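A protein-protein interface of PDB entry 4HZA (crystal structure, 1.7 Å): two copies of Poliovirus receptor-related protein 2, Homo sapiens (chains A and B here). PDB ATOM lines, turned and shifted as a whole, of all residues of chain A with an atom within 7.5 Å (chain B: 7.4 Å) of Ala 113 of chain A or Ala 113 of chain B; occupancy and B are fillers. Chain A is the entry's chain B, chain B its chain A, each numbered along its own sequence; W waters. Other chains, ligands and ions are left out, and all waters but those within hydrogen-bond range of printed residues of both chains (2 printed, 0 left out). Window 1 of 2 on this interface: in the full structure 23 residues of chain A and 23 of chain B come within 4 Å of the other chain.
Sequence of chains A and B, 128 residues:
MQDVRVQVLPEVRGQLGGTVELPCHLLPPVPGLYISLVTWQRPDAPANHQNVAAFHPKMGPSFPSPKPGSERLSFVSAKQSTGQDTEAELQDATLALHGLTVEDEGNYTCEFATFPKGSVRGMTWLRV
OE2 of Glu 111 of chain A lies close to OE1 of Glu 111 of chain B (2.9 Å). The side-chain carboxylate (OE1) of Glu 111 of chain B is in hydrogen-bond range of the side-chain hydroxyl (OG) of Ser 119 of chain A (3.3 Å). The side-chain hydroxyl (OG) of Ser 36 of chain B lies close to a ring nitrogen (NE2) of His 56 of chain A (3.4 Å). The side-chain hydroxyl of Ser 119 of chain B sits at hydrogen-bond distance from the side-chain carboxylate of Glu 111 of chain A (3.3 Å).
O of Thr 39 of chain A sits at hydrogen-bond distance from N of Glu 111 of chain A (2.7 Å). The side-chain hydroxyl (OG1) of Thr 114 of chain A sits at hydrogen-bond distance from the backbone carbonyl oxygen (O) of Gly 118 of chain A (2.7 Å). O of Leu 37 of chain B is in hydrogen-bond range of N of Ala 113 of chain B (2.8 Å).
His 56 of chain B touches Ser 36 of chain A. C of Ala 113 of chain B touches CD2 of Leu 37 of chain A, at 3.7 Å. Gly 118 of chain B touches Thr 39 of chain A. CD1 of Phe 115 of chain B touches CB of His 56 of chain A (3.5 Å). C of Ala 113 of chain A touches CD2 of Leu 37 of chain B, at 3.8 Å. Ala 113 of chain A touches Ala 113 of chain B. Thr 114 of chain A touches Leu 37 of chain B (O to CD2, 3.2 Å). Phe 115 of chain A touches His 56 of chain B (CD1 to CB, 3.6 Å).
Printed residues of chain B within 4 Å of Thr 39 of chain A: Gly 118 and Ser 119. Printed residues of chain B within 4 Å of His 56 of chain A: Ser 36 and Phe 115. Ala 113 of chain A touches just these residues of chain B: Leu 37 and Ala 113. Printed residues of chain A within 4 Å of His 56 of chain B: Tyr 34 (3.0 Å), Ser 36 (3.4 Å) and Phe 115 (3.6 Å). Ala 113 of chain B touches just these residues of chain A: Leu 37 and Ala 113. The nearest printed residue of chain B that does not touch Ala 113 of chain A is Glu 111 of chain B (5.5 Å).
Printed residues of chain A that touch a printed residue of chain B: Tyr 34, Ser 36, Leu 37, Thr 39, His 56, Glu 111, Ala 113, Thr 114, Phe 115 and Ser 119. Along chain A the printed residues that touch a printed residue of chain B span positions 34 to 119. Hydrophobic or aromatic side chains of chain B within 4 Å of the printed part of chain A: Leu 37, His 56, Ala 113 and Phe 115. Among the printed residues, no Asp or Glu carboxylate lies within 4 Å of a Lys or Arg side-chain nitrogen of the other chain.
Tyr 34 of chain A touches His 56 of chain B, but with the chains exchanged His 56 of chain A does not touch Tyr 34 of chain B (5.6 Å). Ser 36 of chain B touches its own counterpart, Ser 36 of chain A. Ser 36 of chain A touches His 56 of chain B, and with the chains exchanged His 56 of chain A touches Ser 36 of chain B. Positions printed for both chains: 26, 33, 34, 35, 36, 37, 38, 39, 56, 90, 111, 112, 113, 114, 115, 117, 118, 119 and 120.
Water W1 bridges a ring nitrogen (NE2) of His 56 of chain A and the side-chain hydroxyl (OG) of Ser 36 of chain B. Water W2 lies within hydrogen-bond range of the side-chain hydroxyl of Thr 39 of chain A (3.1 Å), the backbone carbonyl oxygen of Glu 111 of chain A (3.3 Å) and the side-chain hydroxyl of Ser 119 of chain B (3.4 Å).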
ATOM      1  N   LEU A  26      -4.266  17.949  12.839  1.00  0.00           N
ATOM      2  CA  LEU A  26      -3.979  16.875  11.907  1.00  0.00           C
ATOM      3  C   LEU A  26      -3.770  17.502  10.494  1.00  0.00           C
ATOM      4  O   LEU A  26      -4.636  18.207  10.031  1.00  0.00           O
ATOM      5  CB  LEU A  26      -5.126  15.846  11.885  1.00  0.00           C
ATOM      6  CG  LEU A  26      -4.891  14.695  10.906  1.00  0.00           C
ATOM      7  CD1 LEU A  26      -3.745  13.808  11.419  1.00  0.00           C
ATOM      8  CD2 LEU A  26      -6.149  13.915  10.825  1.00  0.00           C
ATOM      9  N   LEU A  33     -10.339  11.479   3.954  1.00  0.00           N
ATOM     10  CA  LEU A  33      -9.863  11.065   5.281  1.00  0.00           C
ATOM     11  C   LEU A  33     -10.902  11.277   6.406  1.00  0.00           C
ATOM     12  O   LEU A  33     -11.302  12.392   6.643  1.00  0.00           O
ATOM     13  CB  LEU A  33      -8.532  11.767   5.597  1.00  0.00           C
ATOM     14  CG  LEU A  33      -7.865  11.192   6.880  1.00  0.00           C
ATOM     15  CD1 LEU A  33      -7.510   9.728   6.737  1.00  0.00           C
ATOM     16  CD2 LEU A  33      -6.603  11.954   7.177  1.00  0.00           C
ATOM     17  N   TYR A  34     -11.376  10.207   7.085  1.00  0.00           N
ATOM     18  CA  TYR A  34     -12.371  10.329   8.177  1.00  0.00           C
ATOM     19  C   TYR A  34     -11.587  10.348   9.487  1.00  0.00           C
ATOM     20  O   TYR A  34     -10.738   9.480   9.721  1.00  0.00           O
ATOM     21  CB  TYR A  34     -13.322   9.109   8.234  1.00  0.00           C
ATOM     22  CG  TYR A  34     -14.479   9.103   9.307  1.00  0.00           C
ATOM     23  CD1 TYR A  34     -15.498  10.052   9.254  1.00  0.00           C
ATOM     24  CD2 TYR A  34     -14.584   8.079  10.322  1.00  0.00           C
ATOM     25  CE1 TYR A  34     -16.548  10.045  10.175  1.00  0.00           C
ATOM     26  CE2 TYR A  34     -15.648   8.076  11.299  1.00  0.00           C
ATOM     27  CZ  TYR A  34     -16.630   9.074  11.168  1.00  0.00           C
ATOM     28  OH  TYR A  34     -17.729   9.191  12.015  1.00  0.00           O
ATOM     29  N   ILE A  35     -11.897  11.308  10.336  1.00  0.00           N
ATOM     30  CA  ILE A  35     -11.369  11.360  11.682  1.00  0.00           C
ATOM     31  C   ILE A  35     -12.393  10.734  12.611  1.00  0.00           C
ATOM     32  O   ILE A  35     -13.456  11.353  12.873  1.00  0.00           O
ATOM     33  CB  ILE A  35     -11.055  12.815  12.164  1.00  0.00           C
ATOM     34  CG1 ILE A  35      -9.966  13.408  11.235  1.00  0.00           C
ATOM     35  CG2 ILE A  35     -10.517  12.743  13.606  1.00  0.00           C
ATOM     36  CD1 ILE A  35      -9.714  15.004  11.403  1.00  0.00           C
ATOM     37  N   SER A  36     -12.090   9.535  13.102  1.00  0.00           N
ATOM     38  CA  SER A  36     -12.998   8.725  13.897  1.00  0.00           C
ATOM     39  C   SER A  36     -13.021   9.143  15.321  1.00  0.00           C
ATOM     40  O   SER A  36     -14.053   8.973  15.999  1.00  0.00           O
ATOM     41  CB  SER A  36     -12.692   7.219  13.755  1.00  0.00           C
ATOM     42  OG  SER A  36     -12.882   6.858  12.393  1.00  0.00           O
ATOM     43  N   LEU A  37     -11.861   9.564  15.833  1.00  0.00           N
ATOM     44  CA  LEU A  37     -11.807   9.968  17.277  1.00  0.00           C
ATOM     45  C   LEU A  37     -10.514  10.754  17.453  1.00  0.00           C
ATOM     46  O   LEU A  37      -9.504  10.506  16.746  1.00  0.00           O
ATOM     47  CB  LEU A  37     -11.699   8.675  18.136  1.00  0.00           C
ATOM     48  CG  LEU A  37     -11.915   8.889  19.647  1.00  0.00           C
ATOM     49  CD1 LEU A  37     -13.415   9.040  19.954  1.00  0.00           C
ATOM     50  CD2 LEU A  37     -11.427   7.704  20.487  1.00  0.00           C
ATOM     51  N   VAL A  38     -10.534  11.708  18.388  1.00  0.00           N
ATOM     52  CA  VAL A  38      -9.286  12.311  18.874  1.00  0.00           C
ATOM     53  C   VAL A  38      -9.177  11.932  20.318  1.00  0.00           C
ATOM     54  O   VAL A  38     -10.168  11.901  21.036  1.00  0.00           O
ATOM     55  CB  VAL A  38      -9.262  13.874  18.880  1.00  0.00           C
ATOM     56  CG1 VAL A  38      -7.819  14.409  19.332  1.00  0.00           C
ATOM     57  CG2 VAL A  38      -9.611  14.411  17.544  1.00  0.00           C
ATOM     58  N   THR A  39      -7.953  11.658  20.768  1.00  0.00           N
ATOM     59  CA  THR A  39      -7.776  11.481  22.232  1.00  0.00           C
ATOM     60  C   THR A  39      -6.494  12.168  22.681  1.00  0.00           C
ATOM     61  O   THR A  39      -5.519  12.262  21.935  1.00  0.00           O
ATOM     62  CB  THR A  39      -7.642   9.971  22.691  1.00  0.00           C
ATOM     63  OG1 THR A  39      -6.544   9.437  22.007  1.00  0.00           O
ATOM     64  CG2 THR A  39      -8.760   9.074  22.216  1.00  0.00           C
ATOM     65  N   HIS A  56     -15.493  12.667  19.956  1.00  0.00           N
ATOM     66  CA  HIS A  56     -16.063  11.831  18.912  1.00  0.00           C
ATOM     67  C   HIS A  56     -16.907  12.720  17.981  1.00  0.00           C
ATOM     68  O   HIS A  56     -17.574  13.621  18.500  1.00  0.00           O
ATOM     69  CB  HIS A  56     -16.938  10.827  19.638  1.00  0.00           C
ATOM     70  CG  HIS A  56     -17.514   9.790  18.734  1.00  0.00           C
ATOM     71  ND1 HIS A  56     -18.624  10.035  17.953  1.00  0.00           N
ATOM     72  CD2 HIS A  56     -17.199   8.493  18.543  1.00  0.00           C
ATOM     73  CE1 HIS A  56     -18.917   8.954  17.250  1.00  0.00           C
ATOM     74  NE2 HIS A  56     -18.058   8.003  17.582  1.00  0.00           N
ATOM     75  N   LEU A  90     -12.926  17.885  13.603  1.00  0.00           N
ATOM     76  CA  LEU A  90     -12.030  17.369  14.612  1.00  0.00           C
ATOM     77  C   LEU A  90     -10.558  17.639  14.243  1.00  0.00           C
ATOM     78  O   LEU A  90      -9.687  17.305  15.027  1.00  0.00           O
ATOM     79  CB  LEU A  90     -12.191  15.839  14.731  1.00  0.00           C
ATOM     80  CG  LEU A  90     -13.127  15.463  15.864  1.00  0.00           C
ATOM     81  CD1 LEU A  90     -14.569  15.872  15.562  1.00  0.00           C
ATOM     82  CD2 LEU A  90     -13.048  13.966  16.072  1.00  0.00           C
ATOM     83  N   GLU A 111      -3.698  12.218  19.882  1.00  0.00           N
ATOM     84  CA  GLU A 111      -3.755  11.129  18.852  1.00  0.00           C
ATOM     85  C   GLU A 111      -5.046  11.260  18.045  1.00  0.00           C
ATOM     86  O   GLU A 111      -6.104  11.554  18.598  1.00  0.00           O
ATOM     87  CB  GLU A 111      -3.668   9.773  19.552  1.00  0.00           C
ATOM     88  CG  GLU A 111      -3.945   8.599  18.558  1.00  0.00           C
ATOM     89  CD  GLU A 111      -3.732   7.204  19.234  1.00  0.00           C
ATOM     90  OE1 GLU A 111      -4.095   6.991  20.416  1.00  0.00           O
ATOM     91  OE2 GLU A 111      -3.154   6.317  18.585  1.00  0.00           O
ATOM     92  N   PHE A 112      -4.957  10.988  16.746  1.00  0.00           N
ATOM     93  CA  PHE A 112      -6.083  10.976  15.825  1.00  0.00           C
ATOM     94  C   PHE A 112      -6.215   9.546  15.325  1.00  0.00           C
ATOM     95  O   PHE A 112      -5.195   8.979  14.853  1.00  0.00           O
ATOM     96  CB  PHE A 112      -5.798  11.870  14.564  1.00  0.00           C
ATOM     97  CG  PHE A 112      -5.812  13.344  14.886  1.00  0.00           C
ATOM     98  CD1 PHE A 112      -4.642  13.952  15.320  1.00  0.00           C
ATOM     99  CD2 PHE A 112      -6.971  14.093  14.786  1.00  0.00           C
ATOM    100  CE1 PHE A 112      -4.621  15.301  15.638  1.00  0.00           C
ATOM    101  CE2 PHE A 112      -6.973  15.486  15.163  1.00  0.00           C
ATOM    102  CZ  PHE A 112      -5.821  16.062  15.541  1.00  0.00           C
ATOM    103  N   ALA A 113      -7.417   8.988  15.490  1.00  0.00           N
ATOM    104  CA  ALA A 113      -7.739   7.642  14.917  1.00  0.00           C
ATOM    105  C   ALA A 113      -8.461   7.925  13.633  1.00  0.00           C
ATOM    106  O   ALA A 113      -9.507   8.532  13.670  1.00  0.00           O
ATOM    107  CB  ALA A 113      -8.625   6.923  15.935  1.00  0.00           C
ATOM    108  N   THR A 114      -7.873   7.552  12.512  1.00  0.00           N
ATOM    109  CA  THR A 114      -8.433   7.982  11.222  1.00  0.00           C
ATOM    110  C   THR A 114      -8.609   6.747  10.388  1.00  0.00           C
ATOM    111  O   THR A 114      -7.967   5.676  10.571  1.00  0.00           O
ATOM    112  CB  THR A 114      -7.460   8.940  10.429  1.00  0.00           C
ATOM    113  OG1 THR A 114      -6.379   8.214   9.835  1.00  0.00           O
ATOM    114  CG2 THR A 114      -6.954  10.148  11.298  1.00  0.00           C
ATOM    115  N   PHE A 115      -9.438   6.929   9.382  1.00  0.00           N
ATOM    116  CA  PHE A 115      -9.664   5.825   8.411  1.00  0.00           C
ATOM    117  C   PHE A 115      -9.598   6.436   7.010  1.00  0.00           C
ATOM    118  O   PHE A 115     -10.280   7.437   6.752  1.00  0.00           O
ATOM    119  CB  PHE A 115     -11.049   5.156   8.649  1.00  0.00           C
ATOM    120  CG  PHE A 115     -11.269   3.963   7.766  1.00  0.00           C
ATOM    121  CD1 PHE A 115     -10.861   2.720   8.174  1.00  0.00           C
ATOM    122  CD2 PHE A 115     -11.824   4.103   6.505  1.00  0.00           C
ATOM    123  CE1 PHE A 115     -11.076   1.614   7.347  1.00  0.00           C
ATOM    124  CE2 PHE A 115     -12.016   2.994   5.678  1.00  0.00           C
ATOM    125  CZ  PHE A 115     -11.646   1.797   6.077  1.00  0.00           C
ATOM    126  N   LYS A 117      -6.283   5.685   7.016  1.00  0.00           N
ATOM    127  CA  LYS A 117      -4.838   5.741   7.237  1.00  0.00           C
ATOM    128  C   LYS A 117      -4.364   5.219   8.613  1.00  0.00           C
ATOM    129  O   LYS A 117      -3.182   4.939   8.778  1.00  0.00           O
ATOM    130  CB  LYS A 117      -4.348   7.203   7.016  1.00  0.00           C
ATOM    131  CG  LYS A 117      -4.600   7.776   5.584  1.00  0.00           C
ATOM    132  CD  LYS A 117      -3.289   7.786   4.766  1.00  0.00           C
ATOM    133  CE  LYS A 117      -3.499   7.548   3.262  1.00  0.00           C
ATOM    134  NZ  LYS A 117      -2.229   7.269   2.516  1.00  0.00           N
ATOM    135  N   GLY A 118      -5.261   5.122   9.591  1.00  0.00           N
ATOM    136  CA  GLY A 118      -4.943   4.582  10.928  1.00  0.00           C
ATOM    137  C   GLY A 118      -4.694   5.704  11.956  1.00  0.00           C
ATOM    138  O   GLY A 118      -5.167   6.827  11.795  1.00  0.00           O
ATOM    139  N   SER A 119      -3.867   5.414  12.928  1.00  0.00           N
ATOM    140  CA  SER A 119      -3.653   6.345  14.064  1.00  0.00           C
ATOM    141  C   SER A 119      -2.349   7.062  13.946  1.00  0.00           C
ATOM    142  O   SER A 119      -1.301   6.454  13.640  1.00  0.00           O
ATOM    143  CB  SER A 119      -3.755   5.533  15.372  1.00  0.00           C
ATOM    144  OG  SER A 119      -5.164   5.346  15.501  1.00  0.00           O
ATOM    145  N   VAL A 120      -2.363   8.330  14.352  1.00  0.00           N
ATOM    146  CA  VAL A 120      -1.104   9.098  14.355  1.00  0.00           C
ATOM    147  C   VAL A 120      -1.145   9.955  15.610  1.00  0.00           C
ATOM    148  O   VAL A 120      -2.216  10.324  16.110  1.00  0.00           O
ATOM    149  CB  VAL A 120      -0.957   9.988  13.153  1.00  0.00           C
ATOM    150  CG1 VAL A 120      -0.524   9.147  11.948  1.00  0.00           C
ATOM    151  CG2 VAL A 120      -2.189  10.773  12.846  1.00  0.00           C
ATOM    152  N   LEU B  26     -10.952  -6.569  23.236  1.00  0.00           N
ATOM    153  CA  LEU B  26     -11.218  -5.514  24.237  1.00  0.00           C
ATOM    154  C   LEU B  26     -12.144  -6.083  25.291  1.00  0.00           C
ATOM    155  O   LEU B  26     -13.248  -6.597  24.931  1.00  0.00           O
ATOM    156  CB  LEU B  26     -11.849  -4.266  23.539  1.00  0.00           C
ATOM    157  CG  LEU B  26     -12.187  -3.032  24.450  1.00  0.00           C
ATOM    158  CD1 LEU B  26     -10.858  -2.308  24.808  1.00  0.00           C
ATOM    159  CD2 LEU B  26     -13.083  -2.064  23.699  1.00  0.00           C
ATOM    160  N   LEU B  33     -20.295   1.867  25.838  1.00  0.00           N
ATOM    161  CA  LEU B  33     -18.937   1.970  25.292  1.00  0.00           C
ATOM    162  C   LEU B  33     -18.964   1.637  23.818  1.00  0.00           C
ATOM    163  O   LEU B  33     -19.467   0.567  23.414  1.00  0.00           O
ATOM    164  CB  LEU B  33     -17.977   1.058  26.036  1.00  0.00           C
ATOM    165  CG  LEU B  33     -16.517   1.335  25.654  1.00  0.00           C
ATOM    166  CD1 LEU B  33     -15.695   1.115  26.865  1.00  0.00           C
ATOM    167  CD2 LEU B  33     -16.063   0.449  24.497  1.00  0.00           C
ATOM    168  N   TYR B  34     -18.465   2.563  22.999  1.00  0.00           N
ATOM    169  CA  TYR B  34     -18.392   2.366  21.574  1.00  0.00           C
ATOM    170  C   TYR B  34     -16.986   2.228  21.091  1.00  0.00           C
ATOM    171  O   TYR B  34     -16.142   3.023  21.468  1.00  0.00           O
ATOM    172  CB  TYR B  34     -19.044   3.539  20.822  1.00  0.00           C
ATOM    173  CG  TYR B  34     -20.498   3.583  21.148  1.00  0.00           C
ATOM    174  CD1 TYR B  34     -20.954   4.191  22.327  1.00  0.00           C
ATOM    175  CD2 TYR B  34     -21.455   3.006  20.259  1.00  0.00           C
ATOM    176  CE1 TYR B  34     -22.378   4.188  22.653  1.00  0.00           C
ATOM    177  CE2 TYR B  34     -22.849   3.019  20.561  1.00  0.00           C
ATOM    178  CZ  TYR B  34     -23.287   3.601  21.757  1.00  0.00           C
ATOM    179  OH  TYR B  34     -24.640   3.601  22.055  1.00  0.00           O
ATOM    180  N   ILE B  35     -16.791   1.308  20.134  1.00  0.00           N
ATOM    181  CA  ILE B  35     -15.474   1.204  19.530  1.00  0.00           C
ATOM    182  C   ILE B  35     -15.588   1.956  18.234  1.00  0.00           C
ATOM    183  O   ILE B  35     -16.310   1.493  17.332  1.00  0.00           O
ATOM    184  CB  ILE B  35     -15.071  -0.280  19.259  1.00  0.00           C
ATOM    185  CG1 ILE B  35     -15.199  -1.091  20.578  1.00  0.00           C
ATOM    186  CG2 ILE B  35     -13.707  -0.287  18.568  1.00  0.00           C
ATOM    187  CD1 ILE B  35     -14.796  -2.581  20.528  1.00  0.00           C
ATOM    188  N   SER B  36     -14.845   3.041  18.105  1.00  0.00           N
ATOM    189  CA  SER B  36     -14.884   3.942  16.942  1.00  0.00           C
ATOM    190  C   SER B  36     -13.931   3.465  15.855  1.00  0.00           C
ATOM    191  O   SER B  36     -14.192   3.773  14.684  1.00  0.00           O
ATOM    192  CB  SER B  36     -14.555   5.404  17.322  1.00  0.00           C
ATOM    193  OG  SER B  36     -15.493   5.831  18.303  1.00  0.00           O
ATOM    194  N   LEU B  37     -12.826   2.804  16.249  1.00  0.00           N
ATOM    195  CA  LEU B  37     -11.854   2.321  15.271  1.00  0.00           C
ATOM    196  C   LEU B  37     -10.962   1.296  15.988  1.00  0.00           C
ATOM    197  O   LEU B  37     -10.684   1.476  17.173  1.00  0.00           O
ATOM    198  CB  LEU B  37     -10.996   3.461  14.748  1.00  0.00           C
ATOM    199  CG  LEU B  37     -10.108   3.192  13.490  1.00  0.00           C
ATOM    200  CD1 LEU B  37     -11.057   3.141  12.277  1.00  0.00           C
ATOM    201  CD2 LEU B  37      -9.152   4.231  13.204  1.00  0.00           C
ATOM    202  N   VAL B  38     -10.531   0.269  15.250  1.00  0.00           N
ATOM    203  CA  VAL B  38      -9.435  -0.584  15.739  1.00  0.00           C
ATOM    204  C   VAL B  38      -8.251  -0.344  14.806  1.00  0.00           C
ATOM    205  O   VAL B  38      -8.434  -0.212  13.567  1.00  0.00           O
ATOM    206  CB  VAL B  38      -9.891  -2.114  15.592  1.00  0.00           C
ATOM    207  CG1 VAL B  38      -8.710  -3.009  15.818  1.00  0.00           C
ATOM    208  CG2 VAL B  38     -10.968  -2.438  16.551  1.00  0.00           C
ATOM    209  N   THR B  39      -7.017  -0.357  15.329  1.00  0.00           N
ATOM    210  CA  THR B  39      -5.843  -0.178  14.446  1.00  0.00           C
ATOM    211  C   THR B  39      -4.742  -1.115  14.912  1.00  0.00           C
ATOM    212  O   THR B  39      -4.532  -1.270  16.126  1.00  0.00           O
ATOM    213  CB  THR B  39      -5.268   1.248  14.454  1.00  0.00           C
ATOM    214  OG1 THR B  39      -4.807   1.571  15.767  1.00  0.00           O
ATOM    215  CG2 THR B  39      -6.301   2.302  14.070  1.00  0.00           C
ATOM    216  N   HIS B  56     -13.019   0.004  10.613  1.00  0.00           N
ATOM    217  CA  HIS B  56     -13.976   1.052  10.995  1.00  0.00           C
ATOM    218  C   HIS B  56     -15.367   0.347  11.093  1.00  0.00           C
ATOM    219  O   HIS B  56     -15.702  -0.511  10.250  1.00  0.00           O
ATOM    220  CB  HIS B  56     -13.986   2.129   9.928  1.00  0.00           C
ATOM    221  CG  HIS B  56     -14.929   3.273  10.205  1.00  0.00           C
ATOM    222  ND1 HIS B  56     -16.277   3.213   9.970  1.00  0.00           N
ATOM    223  CD2 HIS B  56     -14.678   4.524  10.665  1.00  0.00           C
ATOM    224  CE1 HIS B  56     -16.836   4.357  10.320  1.00  0.00           C
ATOM    225  NE2 HIS B  56     -15.885   5.163  10.758  1.00  0.00           N
ATOM    226  N   LEU B  90     -16.518  -5.138  17.024  1.00  0.00           N
ATOM    227  CA  LEU B  90     -15.112  -4.884  16.879  1.00  0.00           C
ATOM    228  C   LEU B  90     -14.365  -5.372  18.117  1.00  0.00           C
ATOM    229  O   LEU B  90     -13.178  -5.264  18.098  1.00  0.00           O
ATOM    230  CB  LEU B  90     -14.851  -3.360  16.695  1.00  0.00           C
ATOM    231  CG  LEU B  90     -14.870  -2.938  15.218  1.00  0.00           C
ATOM    232  CD1 LEU B  90     -16.220  -3.205  14.699  1.00  0.00           C
ATOM    233  CD2 LEU B  90     -14.566  -1.461  15.058  1.00  0.00           C
ATOM    234  N   GLU B 111      -4.762  -1.422  18.946  1.00  0.00           N
ATOM    235  CA  GLU B 111      -5.320  -0.280  19.696  1.00  0.00           C
ATOM    236  C   GLU B 111      -6.796  -0.145  19.376  1.00  0.00           C
ATOM    237  O   GLU B 111      -7.205  -0.262  18.211  1.00  0.00           O
ATOM    238  CB  GLU B 111      -4.650   1.003  19.296  1.00  0.00           C
ATOM    239  CG  GLU B 111      -5.205   2.221  20.089  1.00  0.00           C
ATOM    240  CD  GLU B 111      -4.509   3.492  19.583  1.00  0.00           C
ATOM    241  OE1 GLU B 111      -4.778   3.894  18.415  1.00  0.00           O
ATOM    242  OE2 GLU B 111      -3.663   4.001  20.330  1.00  0.00           O
ATOM    243  N   PHE B 112      -7.609   0.053  20.434  1.00  0.00           N
ATOM    244  CA  PHE B 112      -9.029   0.375  20.260  1.00  0.00           C
ATOM    245  C   PHE B 112      -9.232   1.838  20.545  1.00  0.00           C
ATOM    246  O   PHE B 112      -8.848   2.311  21.618  1.00  0.00           O
ATOM    247  CB  PHE B 112      -9.925  -0.406  21.225  1.00  0.00           C
ATOM    248  CG  PHE B 112      -9.882  -1.938  20.969  1.00  0.00           C
ATOM    249  CD1 PHE B 112      -8.806  -2.669  21.436  1.00  0.00           C
ATOM    250  CD2 PHE B 112     -10.892  -2.552  20.238  1.00  0.00           C
ATOM    251  CE1 PHE B 112      -8.768  -4.068  21.236  1.00  0.00           C
ATOM    252  CE2 PHE B 112     -10.872  -3.909  19.967  1.00  0.00           C
ATOM    253  CZ  PHE B 112      -9.788  -4.677  20.470  1.00  0.00           C
ATOM    254  N   ALA B 113      -9.854   2.558  19.590  1.00  0.00           N
ATOM    255  CA  ALA B 113     -10.172   3.996  19.823  1.00  0.00           C
ATOM    256  C   ALA B 113     -11.592   3.964  20.322  1.00  0.00           C
ATOM    257  O   ALA B 113     -12.495   3.656  19.529  1.00  0.00           O
ATOM    258  CB  ALA B 113     -10.142   4.737  18.503  1.00  0.00           C
ATOM    259  N   THR B 114     -11.818   4.205  21.618  1.00  0.00           N
ATOM    260  CA  THR B 114     -13.186   4.070  22.137  1.00  0.00           C
ATOM    261  C   THR B 114     -13.742   5.332  22.659  1.00  0.00           C
ATOM    262  O   THR B 114     -12.955   6.251  23.035  1.00  0.00           O
ATOM    263  CB  THR B 114     -13.231   3.020  23.353  1.00  0.00           C
ATOM    264  OG1 THR B 114     -12.795   3.614  24.584  1.00  0.00           O
ATOM    265  CG2 THR B 114     -12.331   1.826  23.113  1.00  0.00           C
ATOM    266  N   PHE B 115     -15.095   5.411  22.723  1.00  0.00           N
ATOM    267  CA  PHE B 115     -15.709   6.563  23.346  1.00  0.00           C
ATOM    268  C   PHE B 115     -16.738   5.983  24.314  1.00  0.00           C
ATOM    269  O   PHE B 115     -17.507   5.129  23.928  1.00  0.00           O
ATOM    270  CB  PHE B 115     -16.380   7.428  22.286  1.00  0.00           C
ATOM    271  CG  PHE B 115     -16.908   8.678  22.843  1.00  0.00           C
ATOM    272  CD1 PHE B 115     -16.113   9.793  22.891  1.00  0.00           C
ATOM    273  CD2 PHE B 115     -18.187   8.730  23.395  1.00  0.00           C
ATOM    274  CE1 PHE B 115     -16.580  10.971  23.452  1.00  0.00           C
ATOM    275  CE2 PHE B 115     -18.632   9.929  23.989  1.00  0.00           C
ATOM    276  CZ  PHE B 115     -17.834  11.020  23.974  1.00  0.00           C
ATOM    277  N   LYS B 117     -14.189   6.170  26.657  1.00  0.00           N
ATOM    278  CA  LYS B 117     -12.989   5.884  27.452  1.00  0.00           C
ATOM    279  C   LYS B 117     -11.648   6.255  26.794  1.00  0.00           C
ATOM    280  O   LYS B 117     -10.628   6.314  27.468  1.00  0.00           O
ATOM    281  CB  LYS B 117     -12.944   4.402  27.864  1.00  0.00           C
ATOM    282  CG  LYS B 117     -14.041   4.112  28.903  1.00  0.00           C
ATOM    283  CD  LYS B 117     -13.689   4.692  30.301  1.00  0.00           C
ATOM    284  CE  LYS B 117     -14.673   4.143  31.394  1.00  0.00           C
ATOM    285  NZ  LYS B 117     -14.433   4.761  32.788  1.00  0.00           N
ATOM    286  N   GLY B 118     -11.685   6.510  25.492  1.00  0.00           N
ATOM    287  CA  GLY B 118     -10.442   6.881  24.773  1.00  0.00           C
ATOM    288  C   GLY B 118      -9.691   5.675  24.258  1.00  0.00           C
ATOM    289  O   GLY B 118     -10.275   4.625  24.039  1.00  0.00           O
ATOM    290  N   SER B 119      -8.365   5.803  24.097  1.00  0.00           N
ATOM    291  CA  SER B 119      -7.643   4.805  23.279  1.00  0.00           C
ATOM    292  C   SER B 119      -6.958   3.894  24.229  1.00  0.00           C
ATOM    293  O   SER B 119      -6.286   4.324  25.247  1.00  0.00           O
ATOM    294  CB  SER B 119      -6.549   5.459  22.410  1.00  0.00           C
ATOM    295  OG  SER B 119      -7.149   6.012  21.272  1.00  0.00           O
ATOM    296  N   VAL B 120      -7.032   2.612  23.919  1.00  0.00           N
ATOM    297  CA  VAL B 120      -6.314   1.618  24.781  1.00  0.00           C
ATOM    298  C   VAL B 120      -5.620   0.662  23.862  1.00  0.00           C
ATOM    299  O   VAL B 120      -6.110   0.424  22.790  1.00  0.00           O
ATOM    300  CB  VAL B 120      -7.259   0.919  25.683  1.00  0.00           C
ATOM    301  CG1 VAL B 120      -7.787   1.935  26.692  1.00  0.00           C
ATOM    302  CG2 VAL B 120      -8.458   0.301  24.895  1.00  0.00           C
HETATM  303  O   HOH W   1     -18.093   5.384  16.736  1.00  0.00           O
HETATM  304  O   HOH W   2      -7.788   8.737  19.267  1.00  0.00           O
